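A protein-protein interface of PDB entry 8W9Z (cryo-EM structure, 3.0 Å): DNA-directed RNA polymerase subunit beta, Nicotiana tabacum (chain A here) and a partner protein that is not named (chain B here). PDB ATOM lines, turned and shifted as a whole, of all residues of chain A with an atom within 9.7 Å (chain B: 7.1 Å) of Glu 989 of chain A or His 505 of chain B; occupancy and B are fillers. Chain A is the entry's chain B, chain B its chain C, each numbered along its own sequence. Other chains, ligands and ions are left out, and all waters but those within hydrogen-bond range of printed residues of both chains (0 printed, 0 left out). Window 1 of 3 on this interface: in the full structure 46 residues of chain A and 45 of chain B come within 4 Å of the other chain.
SD of Met 988 of chain A lies close to O of Thr 464 of chain B, at 3.3 Å.
N of Val 998 of chain A sits at hydrogen-bond distance from O of Leu 993 of chain A.
The backbone carbonyl oxygen (O) of Asn 460 of chain B sits at hydrogen-bond distance from the backbone NH (N) of Ala 503 of chain B (3.0 Å).
The side-chain amide oxygen of Asn 460 of chain B lies within hydrogen-bond range of a ring nitrogen (ND1) of His 505 of chain B.
The backbone NH (N) of Leu 458 of chain B lies within hydrogen-bond range of the backbone carbonyl oxygen (O) of His 505 of chain B, 2.9 Å away.
OE2 of Glu 989 of chain A touches CG of Asn 460 of chain B (3.9 Å).
CG1 of Ile 470 of chain B touches CG of Glu 989 of chain A, 3.9 Å away.
Glu 989 of chain A touches His 505 of chain B.
CD1 of Ile 470 of chain B touches CB of Ala 992 of chain A (3.7 Å).
Leu 993 of chain A touches Ile 470 of chain B.
Ile 470 of chain B touches Phe 996 of chain A (O to CE2, 3.6 Å).
OE2 of Glu 1004 of chain A touches C of Pro 507 of chain B, 3.7 Å away.
CE of Met 1005 of chain A touches ND1 of His 505 of chain B, 3.4 Å away.
Of chain B, only Asn 460, Ile 470 and His 505 come within 4 Å of Glu 989 of chain A.
His 505 of chain B touches just these residues of chain A: Glu 989 (3.8 Å) and Met 1005 (3.4 Å).
No residue of chain A comes within 4 Å of Val 457 of chain B.
Of the printed residues of chain B, Phe 996 of chain A touches Ile 470 (3.6 Å).
Of the printed residues of chain A, Pro 507 of chain B touches Glu 1004 (3.7 Å).
Printed residues of chain B within 4 Å of Met 1005 of chain A: His 505 (3.4 Å).
Of the printed residues of chain B, Ala 992 of chain A touches Ile 470.
Of the printed residues of chain A, Thr 464 of chain B touches Met 988.
The nearest printed residue of chain A that does not touch His 505 of chain B is Ile 1001 of chain A (7.2 Å).
The nearest printed residue of chain A that does not touch Ile 470 of chain B is Met 988 of chain A (4.9 Å).
Of the 20 printed residues of chain A, 7 touch a printed residue of chain B.
Hydrophobic or aromatic side chains of chain A within 4 Å of the printed part of chain B: Met 988, Ala 992, Leu 993, Phe 996 and Met 1005.
Printed residues of chain B that touch a printed residue of chain A: Asn 460, Thr 464, Ile 470, His 505 and Pro 507.
Hydrophobic or aromatic side chains of chain B that line the printed part of chain A: Ile 470 and His 505.
Along chain B the printed residues that touch a printed residue of chain A span positions 460 to 507.
Among the printed residues, no Asp or Glu carboxylate lies within 4 Å of a Lys or Arg side-chain nitrogen of the other chain.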
ATOM      1  N   GLY A 986       4.543  31.176  29.247  1.00  0.00           N
ATOM      2  CA  GLY A 986       3.257  31.411  28.620  1.00  0.00           C
ATOM      3  C   GLY A 986       2.862  30.323  27.641  1.00  0.00           C
ATOM      4  O   GLY A 986       3.471  29.255  27.607  1.00  0.00           O
ATOM      5  N   GLU A 987       1.834  30.599  26.837  1.00  0.00           N
ATOM      6  CA  GLU A 987       1.368  29.620  25.861  1.00  0.00           C
ATOM      7  C   GLU A 987       2.303  29.514  24.664  1.00  0.00           C
ATOM      8  O   GLU A 987       2.440  28.429  24.085  1.00  0.00           O
ATOM      9  CB  GLU A 987      -0.047  29.973  25.397  1.00  0.00           C
ATOM     10  CG  GLU A 987      -0.193  31.387  24.858  1.00  0.00           C
ATOM     11  CD  GLU A 987      -1.616  31.712  24.450  1.00  0.00           C
ATOM     12  OE1 GLU A 987      -2.490  30.829  24.583  1.00  0.00           O
ATOM     13  OE2 GLU A 987      -1.862  32.849  23.997  1.00  0.00           O
ATOM     14  N   MET A 988       2.954  30.615  24.282  1.00  0.00           N
ATOM     15  CA  MET A 988       3.851  30.580  23.132  1.00  0.00           C
ATOM     16  C   MET A 988       5.078  29.719  23.410  1.00  0.00           C
ATOM     17  O   MET A 988       5.552  29.000  22.522  1.00  0.00           O
ATOM     18  CB  MET A 988       4.263  32.001  22.746  1.00  0.00           C
ATOM     19  CG  MET A 988       3.101  32.888  22.330  1.00  0.00           C
ATOM     20  SD  MET A 988       3.622  34.556  21.883  1.00  0.00           S
ATOM     21  CE  MET A 988       4.362  35.103  23.419  1.00  0.00           C
ATOM     22  N   GLU A 989       5.597  29.767  24.639  1.00  0.00           N
ATOM     23  CA  GLU A 989       6.733  28.921  24.988  1.00  0.00           C
ATOM     24  C   GLU A 989       6.348  27.446  24.963  1.00  0.00           C
ATOM     25  O   GLU A 989       7.130  26.602  24.512  1.00  0.00           O
ATOM     26  CB  GLU A 989       7.279  29.313  26.359  1.00  0.00           C
ATOM     27  CG  GLU A 989       8.507  28.528  26.788  1.00  0.00           C
ATOM     28  CD  GLU A 989       9.050  28.980  28.129  1.00  0.00           C
ATOM     29  OE1 GLU A 989       8.468  29.912  28.723  1.00  0.00           O
ATOM     30  OE2 GLU A 989      10.060  28.406  28.588  1.00  0.00           O
ATOM     31  N   VAL A 990       5.142  27.120  25.435  1.00  0.00           N
ATOM     32  CA  VAL A 990       4.673  25.739  25.383  1.00  0.00           C
ATOM     33  C   VAL A 990       4.506  25.288  23.938  1.00  0.00           C
ATOM     34  O   VAL A 990       4.860  24.157  23.582  1.00  0.00           O
ATOM     35  CB  VAL A 990       3.366  25.590  26.180  1.00  0.00           C
ATOM     36  CG1 VAL A 990       2.828  24.174  26.061  1.00  0.00           C
ATOM     37  CG2 VAL A 990       3.592  25.956  27.638  1.00  0.00           C
ATOM     38  N   TRP A 991       3.970  26.162  23.083  1.00  0.00           N
ATOM     39  CA  TRP A 991       3.837  25.825  21.669  1.00  0.00           C
ATOM     40  C   TRP A 991       5.198  25.582  21.028  1.00  0.00           C
ATOM     41  O   TRP A 991       5.365  24.640  20.245  1.00  0.00           O
ATOM     42  CB  TRP A 991       3.088  26.937  20.935  1.00  0.00           C
ATOM     43  CG  TRP A 991       1.681  27.126  21.408  1.00  0.00           C
ATOM     44  CD1 TRP A 991       0.953  26.268  22.179  1.00  0.00           C
ATOM     45  CD2 TRP A 991       0.833  28.251  21.151  1.00  0.00           C
ATOM     46  NE1 TRP A 991      -0.297  26.786  22.412  1.00  0.00           N
ATOM     47  CE2 TRP A 991      -0.395  28.003  21.792  1.00  0.00           C
ATOM     48  CE3 TRP A 991       0.994  29.442  20.437  1.00  0.00           C
ATOM     49  CZ2 TRP A 991      -1.457  28.902  21.743  1.00  0.00           C
ATOM     50  CZ3 TRP A 991      -0.062  30.334  20.389  1.00  0.00           C
ATOM     51  CH2 TRP A 991      -1.271  30.059  21.038  1.00  0.00           C
ATOM     52  N   ALA A 992       6.189  26.410  21.365  1.00  0.00           N
ATOM     53  CA  ALA A 992       7.524  26.222  20.805  1.00  0.00           C
ATOM     54  C   ALA A 992       8.154  24.922  21.294  1.00  0.00           C
ATOM     55  O   ALA A 992       8.783  24.199  20.512  1.00  0.00           O
ATOM     56  CB  ALA A 992       8.413  27.414  21.155  1.00  0.00           C
ATOM     57  N   LEU A 993       7.995  24.608  22.582  1.00  0.00           N
ATOM     58  CA  LEU A 993       8.555  23.368  23.112  1.00  0.00           C
ATOM     59  C   LEU A 993       7.878  22.150  22.498  1.00  0.00           C
ATOM     60  O   LEU A 993       8.530  21.126  22.262  1.00  0.00           O
ATOM     61  CB  LEU A 993       8.436  23.344  24.635  1.00  0.00           C
ATOM     62  CG  LEU A 993       9.302  24.345  25.401  1.00  0.00           C
ATOM     63  CD1 LEU A 993       9.105  24.193  26.899  1.00  0.00           C
ATOM     64  CD2 LEU A 993      10.767  24.183  25.033  1.00  0.00           C
ATOM     65  N   GLU A 994       6.572  22.237  22.234  1.00  0.00           N
ATOM     66  CA  GLU A 994       5.890  21.143  21.549  1.00  0.00           C
ATOM     67  C   GLU A 994       6.324  21.040  20.094  1.00  0.00           C
ATOM     68  O   GLU A 994       6.347  19.940  19.531  1.00  0.00           O
ATOM     69  CB  GLU A 994       4.376  21.325  21.640  1.00  0.00           C
ATOM     70  CG  GLU A 994       3.811  21.155  23.040  1.00  0.00           C
ATOM     71  CD  GLU A 994       2.324  21.437  23.104  1.00  0.00           C
ATOM     72  OE1 GLU A 994       1.766  21.931  22.103  1.00  0.00           O
ATOM     73  OE2 GLU A 994       1.711  21.163  24.158  1.00  0.00           O
ATOM     74  N   GLY A 995       6.665  22.168  19.470  1.00  0.00           N
ATOM     75  CA  GLY A 995       7.174  22.122  18.111  1.00  0.00           C
ATOM     76  C   GLY A 995       8.548  21.486  18.026  1.00  0.00           C
ATOM     77  O   GLY A 995       8.839  20.741  17.087  1.00  0.00           O
ATOM     78  N   PHE A 996       9.413  21.772  19.002  1.00  0.00           N
ATOM     79  CA  PHE A 996      10.725  21.134  19.025  1.00  0.00           C
ATOM     80  C   PHE A 996      10.609  19.640  19.300  1.00  0.00           C
ATOM     81  O   PHE A 996      11.369  18.839  18.742  1.00  0.00           O
ATOM     82  CB  PHE A 996      11.624  21.796  20.069  1.00  0.00           C
ATOM     83  CG  PHE A 996      12.275  23.063  19.594  1.00  0.00           C
ATOM     84  CD1 PHE A 996      13.319  23.022  18.688  1.00  0.00           C
ATOM     85  CD2 PHE A 996      11.850  24.293  20.064  1.00  0.00           C
ATOM     86  CE1 PHE A 996      13.922  24.185  18.252  1.00  0.00           C
ATOM     87  CE2 PHE A 996      12.449  25.460  19.632  1.00  0.00           C
ATOM     88  CZ  PHE A 996      13.486  25.405  18.725  1.00  0.00           C
ATOM     89  N   GLY A 997       9.669  19.246  20.150  1.00  0.00           N
ATOM     90  CA  GLY A 997       9.495  17.857  20.511  1.00  0.00           C
ATOM     91  C   GLY A 997      10.032  17.467  21.870  1.00  0.00           C
ATOM     92  O   GLY A 997      10.238  16.273  22.110  1.00  0.00           O
ATOM     93  N   VAL A 998      10.266  18.429  22.760  1.00  0.00           N
ATOM     94  CA  VAL A 998      10.826  18.150  24.083  1.00  0.00           C
ATOM     95  C   VAL A 998       9.645  18.030  25.042  1.00  0.00           C
ATOM     96  O   VAL A 998       9.180  19.008  25.627  1.00  0.00           O
ATOM     97  CB  VAL A 998      11.831  19.215  24.513  1.00  0.00           C
ATOM     98  CG1 VAL A 998      13.185  18.937  23.887  1.00  0.00           C
ATOM     99  CG2 VAL A 998      11.349  20.601  24.104  1.00  0.00           C
ATOM    100  N   ILE A1001      11.029  18.050  28.976  1.00  0.00           N
ATOM    101  CA  ILE A1001      11.360  19.396  29.431  1.00  0.00           C
ATOM    102  C   ILE A1001      10.091  20.190  29.705  1.00  0.00           C
ATOM    103  O   ILE A1001      10.001  20.926  30.695  1.00  0.00           O
ATOM    104  CB  ILE A1001      12.261  20.104  28.402  1.00  0.00           C
ATOM    105  CG1 ILE A1001      13.540  19.299  28.172  1.00  0.00           C
ATOM    106  CG2 ILE A1001      12.595  21.512  28.863  1.00  0.00           C
ATOM    107  CD1 ILE A1001      14.509  19.954  27.216  1.00  0.00           C
ATOM    108  N   LEU A1002       9.087  20.048  28.836  1.00  0.00           N
ATOM    109  CA  LEU A1002       7.817  20.731  29.052  1.00  0.00           C
ATOM    110  C   LEU A1002       7.136  20.238  30.322  1.00  0.00           C
ATOM    111  O   LEU A1002       6.585  21.035  31.091  1.00  0.00           O
ATOM    112  CB  LEU A1002       6.905  20.534  27.842  1.00  0.00           C
ATOM    113  CG  LEU A1002       5.569  21.276  27.862  1.00  0.00           C
ATOM    114  CD1 LEU A1002       5.793  22.778  27.911  1.00  0.00           C
ATOM    115  CD2 LEU A1002       4.732  20.897  26.653  1.00  0.00           C
ATOM    116  N   GLU A1004       8.619  18.919  32.991  1.00  0.00           N
ATOM    117  CA  GLU A1004       9.373  19.436  34.128  1.00  0.00           C
ATOM    118  C   GLU A1004       9.068  20.909  34.370  1.00  0.00           C
ATOM    119  O   GLU A1004       8.900  21.334  35.518  1.00  0.00           O
ATOM    120  CB  GLU A1004      10.871  19.230  33.900  1.00  0.00           C
ATOM    121  CG  GLU A1004      11.751  19.838  34.975  1.00  0.00           C
ATOM    122  CD  GLU A1004      13.228  19.679  34.677  1.00  0.00           C
ATOM    123  OE1 GLU A1004      13.565  18.948  33.723  1.00  0.00           O
ATOM    124  OE2 GLU A1004      14.050  20.287  35.391  1.00  0.00           O
ATOM    125  N   MET A1005       8.985  21.701  33.298  1.00  0.00           N
ATOM    126  CA  MET A1005       8.691  23.122  33.451  1.00  0.00           C
ATOM    127  C   MET A1005       7.295  23.337  34.022  1.00  0.00           C
ATOM    128  O   MET A1005       7.096  24.197  34.889  1.00  0.00           O
ATOM    129  CB  MET A1005       8.837  23.832  32.106  1.00  0.00           C
ATOM    130  CG  MET A1005       8.778  25.347  32.194  1.00  0.00           C
ATOM    131  SD  MET A1005      10.132  26.029  33.168  1.00  0.00           S
ATOM    132  CE  MET A1005      11.545  25.383  32.277  1.00  0.00           C
ATOM    133  N   LEU A1006       6.316  22.557  33.558  1.00  0.00           N
ATOM    134  CA  LEU A1006       4.958  22.696  34.073  1.00  0.00           C
ATOM    135  C   LEU A1006       4.871  22.271  35.534  1.00  0.00           C
ATOM    136  O   LEU A1006       4.171  22.909  36.329  1.00  0.00           O
ATOM    137  CB  LEU A1006       3.984  21.886  33.218  1.00  0.00           C
ATOM    138  CG  LEU A1006       3.229  22.649  32.127  1.00  0.00           C
ATOM    139  CD1 LEU A1006       4.188  23.364  31.189  1.00  0.00           C
ATOM    140  CD2 LEU A1006       2.320  21.708  31.352  1.00  0.00           C
ATOM    141  N   TYR A1008       7.325  22.437  37.689  1.00  0.00           N
ATOM    142  CA  TYR A1008       8.006  23.459  38.477  1.00  0.00           C
ATOM    143  C   TYR A1008       7.144  24.708  38.623  1.00  0.00           C
ATOM    144  O   TYR A1008       7.144  25.348  39.680  1.00  0.00           O
ATOM    145  CB  TYR A1008       9.351  23.804  37.839  1.00  0.00           C
ATOM    146  N   LYS A1009       6.404  25.068  37.571  1.00  0.00           N
ATOM    147  CA  LYS A1009       5.533  26.236  37.647  1.00  0.00           C
ATOM    148  C   LYS A1009       4.321  25.980  38.535  1.00  0.00           C
ATOM    149  O   LYS A1009       3.852  26.897  39.217  1.00  0.00           O
ATOM    150  CB  LYS A1009       5.085  26.651  36.246  1.00  0.00           C
ATOM    151  N   SER B 386      14.852  31.961  37.568  1.00  0.00           N
ATOM    152  CA  SER B 386      14.920  32.698  36.312  1.00  0.00           C
ATOM    153  C   SER B 386      15.151  34.185  36.560  1.00  0.00           C
ATOM    154  O   SER B 386      14.255  34.894  37.018  1.00  0.00           O
ATOM    155  CB  SER B 386      13.639  32.492  35.499  1.00  0.00           C
ATOM    156  N   GLY B 387      16.359  34.650  36.254  1.00  0.00           N
ATOM    157  CA  GLY B 387      16.701  36.045  36.449  1.00  0.00           C
ATOM    158  C   GLY B 387      16.689  36.846  35.165  1.00  0.00           C
ATOM    159  O   GLY B 387      17.566  36.680  34.311  1.00  0.00           O
ATOM    160  N   LEU B 412      21.450  30.038  40.294  1.00  0.00           N
ATOM    161  CA  LEU B 412      20.884  28.893  39.588  1.00  0.00           C
ATOM    162  C   LEU B 412      21.453  27.576  40.104  1.00  0.00           C
ATOM    163  O   LEU B 412      20.703  26.625  40.350  1.00  0.00           O
ATOM    164  CB  LEU B 412      21.130  29.028  38.086  1.00  0.00           C
ATOM    165  CG  LEU B 412      20.316  30.098  37.359  1.00  0.00           C
ATOM    166  CD1 LEU B 412      20.732  30.176  35.903  1.00  0.00           C
ATOM    167  CD2 LEU B 412      18.828  29.812  37.479  1.00  0.00           C
ATOM    168  N   PRO B 456      23.978  21.740  30.416  1.00  0.00           N
ATOM    169  CA  PRO B 456      23.288  22.650  29.497  1.00  0.00           C
ATOM    170  C   PRO B 456      22.277  23.526  30.215  1.00  0.00           C
ATOM    171  O   PRO B 456      21.669  23.132  31.214  1.00  0.00           O
ATOM    172  CB  PRO B 456      22.597  21.699  28.514  1.00  0.00           C
ATOM    173  CG  PRO B 456      22.381  20.455  29.303  1.00  0.00           C
ATOM    174  CD  PRO B 456      23.563  20.340  30.227  1.00  0.00           C
ATOM    175  N   VAL B 457      22.101  24.735  29.687  1.00  0.00           N
ATOM    176  CA  VAL B 457      21.169  25.711  30.232  1.00  0.00           C
ATOM    177  C   VAL B 457      20.287  26.214  29.098  1.00  0.00           C
ATOM    178  O   VAL B 457      20.697  26.249  27.934  1.00  0.00           O
ATOM    179  CB  VAL B 457      21.905  26.878  30.933  1.00  0.00           C
ATOM    180  CG1 VAL B 457      22.523  27.827  29.916  1.00  0.00           C
ATOM    181  CG2 VAL B 457      20.974  27.615  31.878  1.00  0.00           C
ATOM    182  N   LEU B 458      19.057  26.588  29.441  1.00  0.00           N
ATOM    183  CA  LEU B 458      18.070  27.039  28.468  1.00  0.00           C
ATOM    184  C   LEU B 458      17.836  28.536  28.622  1.00  0.00           C
ATOM    185  O   LEU B 458      17.661  29.031  29.740  1.00  0.00           O
ATOM    186  CB  LEU B 458      16.749  26.283  28.629  1.00  0.00           C
ATOM    187  CG  LEU B 458      16.560  24.996  27.822  1.00  0.00           C
ATOM    188  CD1 LEU B 458      17.571  23.935  28.227  1.00  0.00           C
ATOM    189  CD2 LEU B 458      15.141  24.477  27.978  1.00  0.00           C
ATOM    190  N   LEU B 459      17.836  29.247  27.498  1.00  0.00           N
ATOM    191  CA  LEU B 459      17.562  30.677  27.457  1.00  0.00           C
ATOM    192  C   LEU B 459      16.311  30.912  26.624  1.00  0.00           C
ATOM    193  O   LEU B 459      16.191  30.381  25.516  1.00  0.00           O
ATOM    194  CB  LEU B 459      18.742  31.459  26.869  1.00  0.00           C
ATOM    195  CG  LEU B 459      19.979  31.699  27.740  1.00  0.00           C
ATOM    196  CD1 LEU B 459      19.582  32.284  29.086  1.00  0.00           C
ATOM    197  CD2 LEU B 459      20.804  30.431  27.920  1.00  0.00           C
ATOM    198  N   ASN B 460      15.385  31.706  27.155  1.00  0.00           N
ATOM    199  CA  ASN B 460      14.143  32.009  26.460  1.00  0.00           C
ATOM    200  C   ASN B 460      13.790  33.473  26.664  1.00  0.00           C
ATOM    201  O   ASN B 460      13.773  33.959  27.800  1.00  0.00           O
ATOM    202  CB  ASN B 460      13.000  31.111  26.949  1.00  0.00           C
ATOM    203  CG  ASN B 460      12.759  31.229  28.440  1.00  0.00           C
ATOM    204  OD1 ASN B 460      13.433  30.584  29.243  1.00  0.00           O
ATOM    205  ND2 ASN B 460      11.790  32.054  28.819  1.00  0.00           N
ATOM    206  N   ARG B 461      13.518  34.171  25.566  1.00  0.00           N
ATOM    207  CA  ARG B 461      13.080  35.554  25.648  1.00  0.00           C
ATOM    208  C   ARG B 461      11.669  35.629  26.227  1.00  0.00           C
ATOM    209  O   ARG B 461      10.889  34.675  26.157  1.00  0.00           O
ATOM    210  CB  ARG B 461      13.112  36.217  24.270  1.00  0.00           C
ATOM    211  N   ALA B 462      11.348  36.783  26.809  1.00  0.00           N
ATOM    212  CA  ALA B 462      10.001  36.976  27.343  1.00  0.00           C
ATOM    213  C   ALA B 462       8.942  36.972  26.246  1.00  0.00           C
ATOM    214  O   ALA B 462       7.935  36.257  26.398  1.00  0.00           O
ATOM    215  CB  ALA B 462       9.953  38.252  28.192  1.00  0.00           C
ATOM    216  N   THR B 464       7.795  35.319  23.122  1.00  0.00           N
ATOM    217  CA  THR B 464       8.090  34.139  22.308  1.00  0.00           C
ATOM    218  C   THR B 464       7.300  34.184  21.001  1.00  0.00           C
ATOM    219  O   THR B 464       6.437  33.349  20.727  1.00  0.00           O
ATOM    220  CB  THR B 464       7.795  32.866  23.094  1.00  0.00           C
ATOM    221  N   ILE B 470      13.219  29.865  21.983  1.00  0.00           N
ATOM    222  CA  ILE B 470      13.706  29.083  23.114  1.00  0.00           C
ATOM    223  C   ILE B 470      14.826  28.187  22.604  1.00  0.00           C
ATOM    224  O   ILE B 470      14.581  27.245  21.840  1.00  0.00           O
ATOM    225  CB  ILE B 470      12.589  28.258  23.769  1.00  0.00           C
ATOM    226  CG1 ILE B 470      11.503  29.169  24.351  1.00  0.00           C
ATOM    227  CG2 ILE B 470      13.158  27.372  24.862  1.00  0.00           C
ATOM    228  CD1 ILE B 470      10.393  29.529  23.382  1.00  0.00           C
ATOM    229  N   ALA B 503      15.048  35.074  30.281  1.00  0.00           N
ATOM    230  CA  ALA B 503      14.786  34.118  31.347  1.00  0.00           C
ATOM    231  C   ALA B 503      15.728  32.930  31.206  1.00  0.00           C
ATOM    232  O   ALA B 503      15.930  32.418  30.100  1.00  0.00           O
ATOM    233  CB  ALA B 503      13.331  33.652  31.313  1.00  0.00           C
ATOM    234  N   VAL B 504      16.303  32.495  32.324  1.00  0.00           N
ATOM    235  CA  VAL B 504      17.280  31.413  32.342  1.00  0.00           C
ATOM    236  C   VAL B 504      16.684  30.249  33.120  1.00  0.00           C
ATOM    237  O   VAL B 504      16.299  30.405  34.285  1.00  0.00           O
ATOM    238  CB  VAL B 504      18.614  31.861  32.962  1.00  0.00           C
ATOM    239  CG1 VAL B 504      19.735  30.940  32.518  1.00  0.00           C
ATOM    240  CG2 VAL B 504      18.918  33.303  32.587  1.00  0.00           C
ATOM    241  N   HIS B 505      16.609  29.085  32.477  1.00  0.00           N
ATOM    242  CA  HIS B 505      16.086  27.874  33.090  1.00  0.00           C
ATOM    243  C   HIS B 505      17.130  26.768  33.020  1.00  0.00           C
ATOM    244  O   HIS B 505      17.881  26.661  32.046  1.00  0.00           O
ATOM    245  CB  HIS B 505      14.794  27.415  32.401  1.00  0.00           C
ATOM    246  CG  HIS B 505      13.697  28.432  32.437  1.00  0.00           C
ATOM    247  ND1 HIS B 505      12.688  28.470  31.499  1.00  0.00           N
ATOM    248  CD2 HIS B 505      13.449  29.447  33.298  1.00  0.00           C
ATOM    249  CE1 HIS B 505      11.866  29.466  31.780  1.00  0.00           C
ATOM    250  NE2 HIS B 505      12.305  30.074  32.868  1.00  0.00           N
ATOM    251  N   VAL B 506      17.167  25.941  34.059  1.00  0.00           N
ATOM    252  CA  VAL B 506      18.154  24.879  34.199  1.00  0.00           C
ATOM    253  C   VAL B 506      17.419  23.547  34.295  1.00  0.00           C
ATOM    254  O   VAL B 506      16.624  23.346  35.218  1.00  0.00           O
ATOM    255  CB  VAL B 506      19.054  25.090  35.428  1.00  0.00           C
ATOM    256  CG1 VAL B 506      20.045  23.948  35.562  1.00  0.00           C
ATOM    257  CG2 VAL B 506      19.781  26.420  35.332  1.00  0.00           C
ATOM    258  N   PRO B 507      17.639  22.613  33.371  1.00  0.00           N
ATOM    259  CA  PRO B 507      17.011  21.293  33.492  1.00  0.00           C
ATOM    260  C   PRO B 507      17.617  20.489  34.632  1.00  0.00           C
ATOM    261  O   PRO B 507      18.769  20.689  35.025  1.00  0.00           O
ATOM    262  CB  PRO B 507      17.299  20.635  32.137  1.00  0.00           C
ATOM    263  CG  PRO B 507      17.654  21.765  31.221  1.00  0.00           C
ATOM    264  CD  PRO B 507      18.333  22.775  32.085  1.00  0.00           C
